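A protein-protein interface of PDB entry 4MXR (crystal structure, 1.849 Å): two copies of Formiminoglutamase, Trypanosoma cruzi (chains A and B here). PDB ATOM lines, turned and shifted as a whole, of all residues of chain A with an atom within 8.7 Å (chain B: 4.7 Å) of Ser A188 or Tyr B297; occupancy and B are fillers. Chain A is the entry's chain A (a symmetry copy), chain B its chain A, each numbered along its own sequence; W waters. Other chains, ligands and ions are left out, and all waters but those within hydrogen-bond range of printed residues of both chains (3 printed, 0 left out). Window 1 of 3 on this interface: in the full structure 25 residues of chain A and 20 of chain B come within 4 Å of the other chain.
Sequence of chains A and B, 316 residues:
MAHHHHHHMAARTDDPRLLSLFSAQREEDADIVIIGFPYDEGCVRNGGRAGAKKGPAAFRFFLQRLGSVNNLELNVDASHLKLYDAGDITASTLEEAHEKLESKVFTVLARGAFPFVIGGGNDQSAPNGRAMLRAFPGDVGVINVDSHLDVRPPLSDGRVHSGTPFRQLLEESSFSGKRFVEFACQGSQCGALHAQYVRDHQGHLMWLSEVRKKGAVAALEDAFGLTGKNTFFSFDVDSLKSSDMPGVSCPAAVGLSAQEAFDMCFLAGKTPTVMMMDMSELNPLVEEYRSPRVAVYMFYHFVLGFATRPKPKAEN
Among the printed residues, merely in contact across the chains: Gly A187 with Ser B68 (3.5 Å), Gly A187 with Asn B71 (3.4 Å), Ser A188 with Gly B67 (3.7 Å), Ser A188 with Tyr B297 (3.7 Å), Ser A188 with Tyr B300 (3.4 Å), Gln A189 with Ser B68 (3.6 Å), Gln A189 with Tyr B297 (3.6 Å), Ala A253 with Phe B262 (3.9 Å), Ala A253 with Val B294 (3.9 Å) and Val A254 with Phe B262 (3.5 Å).
The guanidinium group (NH2) of Arg B293 sits at hydrogen-bond distance from the backbone carbonyl oxygen (O) of Pro A251. OG of Ser B68 lies within hydrogen-bond range of O of Cys A190, at 3.3 Å. The side-chain amide nitrogen (ND2) of Asn B71 lies close to the backbone NH (N) of Ser A188 (3.5 Å). The backbone carbonyl oxygen of Ser A188 is in hydrogen-bond range of the backbone NH of Ser B68 (3.1 Å). NH2 of Arg B293 lies within hydrogen-bond range of SG of Cys A250 (3.6 Å).
A ring nitrogen (NE2) of His A148 lies within hydrogen-bond range of the side-chain sulfur (SG) of Cys A250 (3.6 Å). The side-chain hydroxyl (OH) of Tyr B300 is in hydrogen-bond range of the backbone carbonyl oxygen (O) of Ser B68, at 2.7 Å. The side-chain amide oxygen (OE1) of Gln A186 is in hydrogen-bond range of the side-chain amide nitrogen (NE2) of Gln A189, 3.1 Å away. O of Ser A147 is in hydrogen-bond range of SG of Cys A190. The backbone carbonyl oxygen (O) of Tyr B297 lies within hydrogen-bond range of a ring nitrogen (ND1) of His B301 (2.8 Å). ND2 of Asn B71 lies within hydrogen-bond range of OH of Tyr B300 (3.1 Å).
Water W2 lies within hydrogen-bond range of the backbone NH of Gly B67 (2.7 Å), the backbone carbonyl oxygen of Ser A188 (2.9 Å) and the side-chain hydroxyl of Tyr B297 (3.4 Å). Water W3 lies within hydrogen-bond range of the backbone carbonyl oxygen of Pro A251 (2.7 Å), the guanidinium group of Arg B293 (2.9 Å) and the backbone NH of Ala A253 (3.3 Å). Water W1 lies within hydrogen-bond range of the side-chain amide oxygen of Gln A189 (2.8 Å), the guanidinium group of Arg B293 (3.0 Å), the side-chain hydroxyl of Tyr B297 (3.0 Å) and the backbone carbonyl oxygen of Pro A251 (3.2 Å).
Of chain B, only Gly B67 (3.7 Å), Ser B68 (3.1 Å), Asn B71 (3.5 Å), Tyr B297 (3.7 Å) and Tyr B300 (3.4 Å) come within 4 Å of Ser A188. Tyr B297 touches just these residues of chain A: Ser A188 (3.7 Å) and Gln A189 (3.6 Å). Printed residues of chain A within 4 Å of Asn B71: Gly A187 (3.4 Å) and Ser A188 (3.5 Å). Of the printed residues of chain B, Gln A189 touches Ser B68 (3.6 Å) and Tyr B297 (3.6 Å). Of the printed residues of chain B, Cys A190 touches Ser B68 (3.3 Å). Of the printed residues of chain A, Arg B293 touches Cys A250 and Pro A251. Of the printed residues of chain A, Ser B68 touches Gly A187 (3.5 Å), Ser A188 (3.1 Å), Gln A189 (3.6 Å) and Cys A190 (3.3 Å). His A148 touches none of the printed residues of chain B. The nearest printed residue of chain B that does not touch Ser A188 is His B301 (4.7 Å). The nearest printed residue of chain A that does not touch Asn B71 is Cys A190 (5.4 Å).
No position is printed for both chains.
Printed residues of chain A that touch a printed residue of chain B: Gly A187, Ser A188, Gln A189, Cys A190, Cys A250, Pro A251, Ala A253 and Val A254. Hydrophobic or aromatic side chains of chain A that line the printed part of chain B: Ala A253 and Val A254.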
ATOM      1  N   SER A 147       5.260  -7.388 -11.091  1.00  0.00           N
ATOM      2  CA  SER A 147       3.981  -8.079 -11.214  1.00  0.00           C
ATOM      3  C   SER A 147       3.918  -8.854 -12.531  1.00  0.00           C
ATOM      4  O   SER A 147       3.120  -9.782 -12.677  1.00  0.00           O
ATOM      5  CB  SER A 147       2.812  -7.094 -11.111  1.00  0.00           C
ATOM      6  OG  SER A 147       2.934  -6.063 -12.074  1.00  0.00           O
ATOM      7  N   HIS A 148       4.765  -8.466 -13.483  1.00  0.00           N
ATOM      8  CA  HIS A 148       4.823  -9.115 -14.797  1.00  0.00           C
ATOM      9  C   HIS A 148       6.143  -9.863 -14.998  1.00  0.00           C
ATOM     10  O   HIS A 148       7.150  -9.537 -14.374  1.00  0.00           O
ATOM     11  CB  HIS A 148       4.641  -8.078 -15.912  1.00  0.00           C
ATOM     12  CG  HIS A 148       3.583  -7.059 -15.618  1.00  0.00           C
ATOM     13  ND1 HIS A 148       3.868  -5.824 -15.074  1.00  0.00           N
ATOM     14  CD2 HIS A 148       2.238  -7.100 -15.773  1.00  0.00           C
ATOM     15  CE1 HIS A 148       2.747  -5.144 -14.915  1.00  0.00           C
ATOM     16  NE2 HIS A 148       1.743  -5.895 -15.331  1.00  0.00           N
ATOM     17  N   ARG A 152       8.327 -11.337 -22.734  1.00  0.00           N
ATOM     18  CA  ARG A 152       7.638 -11.202 -24.009  1.00  0.00           C
ATOM     19  C   ARG A 152       8.634 -11.223 -25.163  1.00  0.00           C
ATOM     20  O   ARG A 152       9.787 -10.810 -25.006  1.00  0.00           O
ATOM     21  CB  ARG A 152       6.831  -9.899 -24.054  1.00  0.00           C
ATOM     22  CG  ARG A 152       5.802  -9.771 -22.947  1.00  0.00           C
ATOM     23  CD  ARG A 152       4.819  -8.646 -23.224  1.00  0.00           C
ATOM     24  NE  ARG A 152       3.886  -8.476 -22.113  1.00  0.00           N
ATOM     25  CZ  ARG A 152       2.809  -9.232 -21.916  1.00  0.00           C
ATOM     26  NH1 ARG A 152       2.517 -10.217 -22.758  1.00  0.00           N
ATOM     27  NH2 ARG A 152       2.024  -9.002 -20.872  1.00  0.00           N
ATOM     28  N   CYS A 185       5.396 -11.850  -8.818  1.00  0.00           N
ATOM     29  CA  CYS A 185       4.644 -11.884 -10.066  1.00  0.00           C
ATOM     30  C   CYS A 185       3.180 -12.229  -9.790  1.00  0.00           C
ATOM     31  O   CYS A 185       2.858 -12.848  -8.773  1.00  0.00           O
ATOM     32  CB  CYS A 185       5.273 -12.871 -11.062  1.00  0.00           C
ATOM     33  SG  CYS A 185       5.718 -14.476 -10.367  1.00  0.00           S
ATOM     34  N   GLN A 186       2.293 -11.817 -10.692  1.00  0.00           N
ATOM     35  CA  GLN A 186       0.860 -11.979 -10.479  1.00  0.00           C
ATOM     36  C   GLN A 186       0.185 -12.829 -11.559  1.00  0.00           C
ATOM     37  O   GLN A 186       0.261 -12.522 -12.749  1.00  0.00           O
ATOM     38  CB  GLN A 186       0.185 -10.609 -10.363  1.00  0.00           C
ATOM     39  CG  GLN A 186       0.664  -9.783  -9.162  1.00  0.00           C
ATOM     40  CD  GLN A 186      -0.033  -8.439  -9.057  1.00  0.00           C
ATOM     41  OE1 GLN A 186      -1.149  -8.270  -9.547  1.00  0.00           O
ATOM     42  NE2 GLN A 186       0.614  -7.481  -8.400  1.00  0.00           N
ATOM     43  N   GLY A 187      -0.483 -13.894 -11.124  1.00  0.00           N
ATOM     44  CA  GLY A 187      -1.106 -14.842 -12.031  1.00  0.00           C
ATOM     45  C   GLY A 187      -2.136 -14.227 -12.958  1.00  0.00           C
ATOM     46  O   GLY A 187      -2.340 -14.707 -14.071  1.00  0.00           O
ATOM     47  N   SER A 188      -2.779 -13.157 -12.503  1.00  0.00           N
ATOM     48  CA  SER A 188      -3.802 -12.491 -13.299  1.00  0.00           C
ATOM     49  C   SER A 188      -3.200 -11.724 -14.473  1.00  0.00           C
ATOM     50  O   SER A 188      -3.916 -11.325 -15.393  1.00  0.00           O
ATOM     51  CB  SER A 188      -4.611 -11.536 -12.421  1.00  0.00           C
ATOM     52  OG  SER A 188      -3.812 -10.447 -12.007  1.00  0.00           O
ATOM     53  N   GLN A 189      -1.883 -11.520 -14.435  1.00  0.00           N
ATOM     54  CA  GLN A 189      -1.196 -10.690 -15.425  1.00  0.00           C
ATOM     55  C   GLN A 189      -0.114 -11.458 -16.178  1.00  0.00           C
ATOM     56  O   GLN A 189       0.518 -10.916 -17.084  1.00  0.00           O
ATOM     57  CB  GLN A 189      -0.546  -9.472 -14.760  1.00  0.00           C
ATOM     58  CG  GLN A 189      -1.417  -8.727 -13.756  1.00  0.00           C
ATOM     59  CD  GLN A 189      -0.916  -7.317 -13.512  1.00  0.00           C
ATOM     60  OE1 GLN A 189      -0.896  -6.490 -14.426  1.00  0.00           O
ATOM     61  NE2 GLN A 189      -0.512  -7.030 -12.275  1.00  0.00           N
ATOM     62  N   CYS A 190       0.112 -12.707 -15.792  1.00  0.00           N
ATOM     63  CA  CYS A 190       1.180 -13.505 -16.389  1.00  0.00           C
ATOM     64  C   CYS A 190       0.614 -14.695 -17.164  1.00  0.00           C
ATOM     65  O   CYS A 190      -0.179 -15.471 -16.633  1.00  0.00           O
ATOM     66  CB  CYS A 190       2.160 -13.980 -15.309  1.00  0.00           C
ATOM     67  SG  CYS A 190       3.039 -12.639 -14.432  1.00  0.00           S
ATOM     68  N   GLY A 191       1.023 -14.838 -18.419  1.00  0.00           N
ATOM     69  CA  GLY A 191       0.492 -15.894 -19.264  1.00  0.00           C
ATOM     70  C   GLY A 191       1.101 -17.266 -19.024  1.00  0.00           C
ATOM     71  O   GLY A 191       2.241 -17.385 -18.571  1.00  0.00           O
ATOM     72  N   TRP A 207       5.178 -16.232  -6.802  1.00  0.00           N
ATOM     73  CA  TRP A 207       3.948 -15.455  -6.927  1.00  0.00           C
ATOM     74  C   TRP A 207       3.728 -14.513  -5.750  1.00  0.00           C
ATOM     75  O   TRP A 207       4.213 -14.756  -4.647  1.00  0.00           O
ATOM     76  CB  TRP A 207       2.737 -16.379  -7.067  1.00  0.00           C
ATOM     77  CG  TRP A 207       2.807 -17.296  -8.251  1.00  0.00           C
ATOM     78  CD1 TRP A 207       3.043 -18.642  -8.232  1.00  0.00           C
ATOM     79  CD2 TRP A 207       2.659 -16.933  -9.629  1.00  0.00           C
ATOM     80  NE1 TRP A 207       3.034 -19.142  -9.514  1.00  0.00           N
ATOM     81  CE2 TRP A 207       2.801 -18.112 -10.390  1.00  0.00           C
ATOM     82  CE3 TRP A 207       2.410 -15.728 -10.296  1.00  0.00           C
ATOM     83  CZ2 TRP A 207       2.708 -18.121 -11.781  1.00  0.00           C
ATOM     84  CZ3 TRP A 207       2.315 -15.739 -11.680  1.00  0.00           C
ATOM     85  CH2 TRP A 207       2.466 -16.928 -12.405  1.00  0.00           C
ATOM     86  N   LEU A 208       2.986 -13.439  -5.995  1.00  0.00           N
ATOM     87  CA  LEU A 208       2.651 -12.484  -4.948  1.00  0.00           C
ATOM     88  C   LEU A 208       2.069 -13.185  -3.722  1.00  0.00           C
ATOM     89  O   LEU A 208       2.507 -12.943  -2.598  1.00  0.00           O
ATOM     90  CB  LEU A 208       1.675 -11.429  -5.479  1.00  0.00           C
ATOM     91  CG  LEU A 208       1.185 -10.382  -4.475  1.00  0.00           C
ATOM     92  CD1 LEU A 208       2.351  -9.563  -3.915  1.00  0.00           C
ATOM     93  CD2 LEU A 208       0.145  -9.481  -5.122  1.00  0.00           C
ATOM     94  N   CYS A 250       1.616   0.766 -15.801  1.00  0.00           N
ATOM     95  CA  CYS A 250       0.675  -0.312 -15.544  1.00  0.00           C
ATOM     96  C   CYS A 250       0.401  -0.451 -14.046  1.00  0.00           C
ATOM     97  O   CYS A 250       1.034  -1.258 -13.364  1.00  0.00           O
ATOM     98  CB  CYS A 250       1.205  -1.627 -16.118  1.00  0.00           C
ATOM     99  SG  CYS A 250      -0.033  -2.935 -16.220  1.00  0.00           S
ATOM    100  N   PRO A 251      -0.554   0.343 -13.532  1.00  0.00           N
ATOM    101  CA  PRO A 251      -0.878   0.369 -12.100  1.00  0.00           C
ATOM    102  C   PRO A 251      -1.392  -0.973 -11.597  1.00  0.00           C
ATOM    103  O   PRO A 251      -2.299  -1.555 -12.195  1.00  0.00           O
ATOM    104  CB  PRO A 251      -1.991   1.423 -12.002  1.00  0.00           C
ATOM    105  CG  PRO A 251      -1.914   2.203 -13.274  1.00  0.00           C
ATOM    106  CD  PRO A 251      -1.421   1.242 -14.309  1.00  0.00           C
ATOM    107  N   ALA A 252      -0.823  -1.450 -10.498  1.00  0.00           N
ATOM    108  CA  ALA A 252      -1.235  -2.724  -9.927  1.00  0.00           C
ATOM    109  C   ALA A 252      -2.427  -2.522  -8.997  1.00  0.00           C
ATOM    110  O   ALA A 252      -2.419  -1.625  -8.157  1.00  0.00           O
ATOM    111  CB  ALA A 252      -0.071  -3.361  -9.178  1.00  0.00           C
ATOM    112  N   ALA A 253      -3.460  -3.343  -9.152  1.00  0.00           N
ATOM    113  CA  ALA A 253      -4.589  -3.292  -8.226  1.00  0.00           C
ATOM    114  C   ALA A 253      -4.130  -3.815  -6.869  1.00  0.00           C
ATOM    115  O   ALA A 253      -4.384  -3.205  -5.830  1.00  0.00           O
ATOM    116  CB  ALA A 253      -5.758  -4.120  -8.756  1.00  0.00           C
ATOM    117  N   VAL A 254      -3.458  -4.960  -6.898  1.00  0.00           N
ATOM    118  CA  VAL A 254      -2.849  -5.554  -5.719  1.00  0.00           C
ATOM    119  C   VAL A 254      -1.339  -5.630  -5.944  1.00  0.00           C
ATOM    120  O   VAL A 254      -0.864  -5.438  -7.065  1.00  0.00           O
ATOM    121  CB  VAL A 254      -3.419  -6.962  -5.450  1.00  0.00           C
ATOM    122  CG1 VAL A 254      -4.897  -6.875  -5.087  1.00  0.00           C
ATOM    123  CG2 VAL A 254      -3.224  -7.861  -6.665  1.00  0.00           C
ATOM    124  N   LEU B  66      -7.744  -7.202 -19.801  1.00  0.00           N
ATOM    125  CA  LEU B  66      -7.236  -7.814 -18.578  1.00  0.00           C
ATOM    126  C   LEU B  66      -7.600  -9.288 -18.385  1.00  0.00           C
ATOM    127  O   LEU B  66      -8.548  -9.796 -18.985  1.00  0.00           O
ATOM    128  CB  LEU B  66      -7.719  -7.020 -17.357  1.00  0.00           C
ATOM    129  CG  LEU B  66      -7.351  -5.538 -17.217  1.00  0.00           C
ATOM    130  CD1 LEU B  66      -8.029  -4.955 -15.977  1.00  0.00           C
ATOM    131  CD2 LEU B  66      -5.839  -5.338 -17.144  1.00  0.00           C
ATOM    132  N   GLY B  67      -6.828  -9.960 -17.533  1.00  0.00           N
ATOM    133  CA  GLY B  67      -7.218 -11.246 -16.980  1.00  0.00           C
ATOM    134  C   GLY B  67      -6.765 -12.480 -17.733  1.00  0.00           C
ATOM    135  O   GLY B  67      -7.487 -12.975 -18.594  1.00  0.00           O
ATOM    136  N   SER B  68      -5.578 -12.981 -17.394  1.00  0.00           N
ATOM    137  CA  SER B  68      -5.051 -14.213 -17.977  1.00  0.00           C
ATOM    138  C   SER B  68      -6.040 -15.366 -17.811  1.00  0.00           C
ATOM    139  O   SER B  68      -6.398 -15.730 -16.689  1.00  0.00           O
ATOM    140  CB  SER B  68      -3.714 -14.585 -17.328  1.00  0.00           C
ATOM    141  OG  SER B  68      -2.758 -13.545 -17.462  1.00  0.00           O
ATOM    142  N   ASN B  71      -4.599 -19.091 -15.188  1.00  0.00           N
ATOM    143  CA  ASN B  71      -3.926 -18.460 -14.062  1.00  0.00           C
ATOM    144  C   ASN B  71      -3.076 -19.459 -13.280  1.00  0.00           C
ATOM    145  O   ASN B  71      -3.595 -20.260 -12.500  1.00  0.00           O
ATOM    146  CB  ASN B  71      -4.959 -17.792 -13.147  1.00  0.00           C
ATOM    147  CG  ASN B  71      -4.320 -17.008 -12.011  1.00  0.00           C
ATOM    148  OD1 ASN B  71      -3.358 -17.460 -11.391  1.00  0.00           O
ATOM    149  ND2 ASN B  71      -4.867 -15.830 -11.723  1.00  0.00           N
ATOM    150  N   PHE B 262     -11.170  -9.672  -4.490  1.00  0.00           N
ATOM    151  CA  PHE B 262     -10.810 -10.725  -5.439  1.00  0.00           C
ATOM    152  C   PHE B 262     -11.072 -12.100  -4.830  1.00  0.00           C
ATOM    153  O   PHE B 262     -11.714 -12.955  -5.445  1.00  0.00           O
ATOM    154  CB  PHE B 262      -9.326 -10.625  -5.821  1.00  0.00           C
ATOM    155  CG  PHE B 262      -8.960  -9.349  -6.536  1.00  0.00           C
ATOM    156  CD1 PHE B 262      -9.937  -8.458  -6.951  1.00  0.00           C
ATOM    157  CD2 PHE B 262      -7.631  -9.050  -6.801  1.00  0.00           C
ATOM    158  CE1 PHE B 262      -9.598  -7.289  -7.606  1.00  0.00           C
ATOM    159  CE2 PHE B 262      -7.284  -7.889  -7.465  1.00  0.00           C
ATOM    160  CZ  PHE B 262      -8.270  -7.003  -7.865  1.00  0.00           C
ATOM    161  N   ARG B 293     -10.438  -0.967 -13.385  1.00  0.00           N
ATOM    162  CA  ARG B 293      -9.531  -2.111 -13.444  1.00  0.00           C
ATOM    163  C   ARG B 293      -9.803  -3.070 -12.288  1.00  0.00           C
ATOM    164  O   ARG B 293      -9.862  -4.286 -12.472  1.00  0.00           O
ATOM    165  CB  ARG B 293      -8.069  -1.650 -13.459  1.00  0.00           C
ATOM    166  CG  ARG B 293      -7.656  -1.016 -14.786  1.00  0.00           C
ATOM    167  CD  ARG B 293      -6.323  -0.277 -14.696  1.00  0.00           C
ATOM    168  NE  ARG B 293      -5.186  -1.180 -14.547  1.00  0.00           N
ATOM    169  CZ  ARG B 293      -4.502  -1.697 -15.564  1.00  0.00           C
ATOM    170  NH1 ARG B 293      -4.838  -1.400 -16.812  1.00  0.00           N
ATOM    171  NH2 ARG B 293      -3.477  -2.507 -15.334  1.00  0.00           N
ATOM    172  N   VAL B 294      -9.986  -2.523 -11.095  1.00  0.00           N
ATOM    173  CA  VAL B 294     -10.338  -3.357  -9.948  1.00  0.00           C
ATOM    174  C   VAL B 294     -11.651  -4.094 -10.193  1.00  0.00           C
ATOM    175  O   VAL B 294     -11.771  -5.294  -9.917  1.00  0.00           O
ATOM    176  CB  VAL B 294     -10.439  -2.527  -8.662  1.00  0.00           C
ATOM    177  CG1 VAL B 294     -11.094  -3.344  -7.548  1.00  0.00           C
ATOM    178  CG2 VAL B 294      -9.049  -2.049  -8.251  1.00  0.00           C
ATOM    179  N   ALA B 295     -12.635  -3.369 -10.718  1.00  0.00           N
ATOM    180  CA  ALA B 295     -13.941  -3.950 -11.018  1.00  0.00           C
ATOM    181  C   ALA B 295     -13.817  -5.111 -12.003  1.00  0.00           C
ATOM    182  O   ALA B 295     -14.450  -6.149 -11.833  1.00  0.00           O
ATOM    183  CB  ALA B 295     -14.881  -2.891 -11.567  1.00  0.00           C
ATOM    184  N   VAL B 296     -13.000  -4.933 -13.036  1.00  0.00           N
ATOM    185  CA  VAL B 296     -12.782  -6.008 -14.003  1.00  0.00           C
ATOM    186  C   VAL B 296     -12.075  -7.209 -13.357  1.00  0.00           C
ATOM    187  O   VAL B 296     -12.455  -8.358 -13.584  1.00  0.00           O
ATOM    188  CB  VAL B 296     -12.021  -5.511 -15.265  1.00  0.00           C
ATOM    189  CG1 VAL B 296     -11.594  -6.681 -16.136  1.00  0.00           C
ATOM    190  CG2 VAL B 296     -12.900  -4.557 -16.065  1.00  0.00           C
ATOM    191  N   TYR B 297     -11.063  -6.944 -12.536  1.00  0.00           N
ATOM    192  CA  TYR B 297     -10.340  -8.021 -11.857  1.00  0.00           C
ATOM    193  C   TYR B 297     -11.249  -8.782 -10.894  1.00  0.00           C
ATOM    194  O   TYR B 297     -11.052  -9.973 -10.657  1.00  0.00           O
ATOM    195  CB  TYR B 297      -9.119  -7.484 -11.108  1.00  0.00           C
ATOM    196  CG  TYR B 297      -7.894  -7.254 -11.970  1.00  0.00           C
ATOM    197  CD1 TYR B 297      -7.371  -8.272 -12.762  1.00  0.00           C
ATOM    198  CD2 TYR B 297      -7.248  -6.023 -11.972  1.00  0.00           C
ATOM    199  CE1 TYR B 297      -6.247  -8.061 -13.544  1.00  0.00           C
ATOM    200  CE2 TYR B 297      -6.127  -5.805 -12.749  1.00  0.00           C
ATOM    201  CZ  TYR B 297      -5.630  -6.822 -13.528  1.00  0.00           C
ATOM    202  OH  TYR B 297      -4.505  -6.591 -14.292  1.00  0.00           O
ATOM    203  N   MET B 298     -12.240  -8.096 -10.332  1.00  0.00           N
ATOM    204  CA  MET B 298     -13.202  -8.760  -9.452  1.00  0.00           C
ATOM    205  C   MET B 298     -14.018  -9.762 -10.253  1.00  0.00           C
ATOM    206  O   MET B 298     -14.162 -10.918  -9.856  1.00  0.00           O
ATOM    207  CB  MET B 298     -14.118  -7.748  -8.753  1.00  0.00           C
ATOM    208  CG  MET B 298     -13.450  -6.999  -7.607  1.00  0.00           C
ATOM    209  SD  MET B 298     -14.422  -5.607  -6.986  1.00  0.00           S
ATOM    210  CE  MET B 298     -15.894  -6.462  -6.437  1.00  0.00           C
ATOM    211  N   PHE B 299     -14.536  -9.310 -11.391  1.00  0.00           N
ATOM    212  CA  PHE B 299     -15.276 -10.175 -12.304  1.00  0.00           C
ATOM    213  C   PHE B 299     -14.382 -11.328 -12.759  1.00  0.00           C
ATOM    214  O   PHE B 299     -14.798 -12.485 -12.794  1.00  0.00           O
ATOM    215  CB  PHE B 299     -15.755  -9.363 -13.512  1.00  0.00           C
ATOM    216  CG  PHE B 299     -16.358 -10.195 -14.607  1.00  0.00           C
ATOM    217  CD1 PHE B 299     -17.617 -10.752 -14.458  1.00  0.00           C
ATOM    218  CD2 PHE B 299     -15.669 -10.413 -15.788  1.00  0.00           C
ATOM    219  CE1 PHE B 299     -18.178 -11.522 -15.465  1.00  0.00           C
ATOM    220  CE2 PHE B 299     -16.224 -11.183 -16.803  1.00  0.00           C
ATOM    221  CZ  PHE B 299     -17.480 -11.735 -16.638  1.00  0.00           C
ATOM    222  N   TYR B 300     -13.142 -10.992 -13.098  1.00  0.00           N
ATOM    223  CA  TYR B 300     -12.150 -11.981 -13.497  1.00  0.00           C
ATOM    224  C   TYR B 300     -11.995 -13.082 -12.455  1.00  0.00           C
ATOM    225  O   TYR B 300     -12.010 -14.266 -12.791  1.00  0.00           O
ATOM    226  CB  TYR B 300     -10.809 -11.294 -13.747  1.00  0.00           C
ATOM    227  CG  TYR B 300      -9.631 -12.234 -13.861  1.00  0.00           C
ATOM    228  CD1 TYR B 300      -9.487 -13.067 -14.963  1.00  0.00           C
ATOM    229  CD2 TYR B 300      -8.655 -12.276 -12.875  1.00  0.00           C
ATOM    230  CE1 TYR B 300      -8.405 -13.920 -15.076  1.00  0.00           C
ATOM    231  CE2 TYR B 300      -7.570 -13.128 -12.979  1.00  0.00           C
ATOM    232  CZ  TYR B 300      -7.451 -13.947 -14.084  1.00  0.00           C
ATOM    233  OH  TYR B 300      -6.369 -14.795 -14.200  1.00  0.00           O
ATOM    234  N   HIS B 301     -11.853 -12.698 -11.189  1.00  0.00           N
ATOM    235  CA  HIS B 301     -11.728 -13.696 -10.130  1.00  0.00           C
ATOM    236  C   HIS B 301     -13.005 -14.526  -9.983  1.00  0.00           C
ATOM    237  O   HIS B 301     -12.941 -15.723  -9.712  1.00  0.00           O
ATOM    238  CB  HIS B 301     -11.281 -13.068  -8.802  1.00  0.00           C
ATOM    239  CG  HIS B 301      -9.808 -12.787  -8.744  1.00  0.00           C
ATOM    240  ND1 HIS B 301      -9.251 -11.635  -9.250  1.00  0.00           N
ATOM    241  CD2 HIS B 301      -8.778 -13.528  -8.269  1.00  0.00           C
ATOM    242  CE1 HIS B 301      -7.938 -11.671  -9.082  1.00  0.00           C
ATOM    243  NE2 HIS B 301      -7.627 -12.807  -8.487  1.00  0.00           N
HETATM  244  O   HOH W   1      -2.569  -4.521 -13.377  1.00  0.00           O
HETATM  245  O   HOH W   2      -4.445  -8.867 -16.792  1.00  0.00           O
HETATM  246  O   HOH W   3      -4.960  -1.977 -11.779  1.00  0.00           O
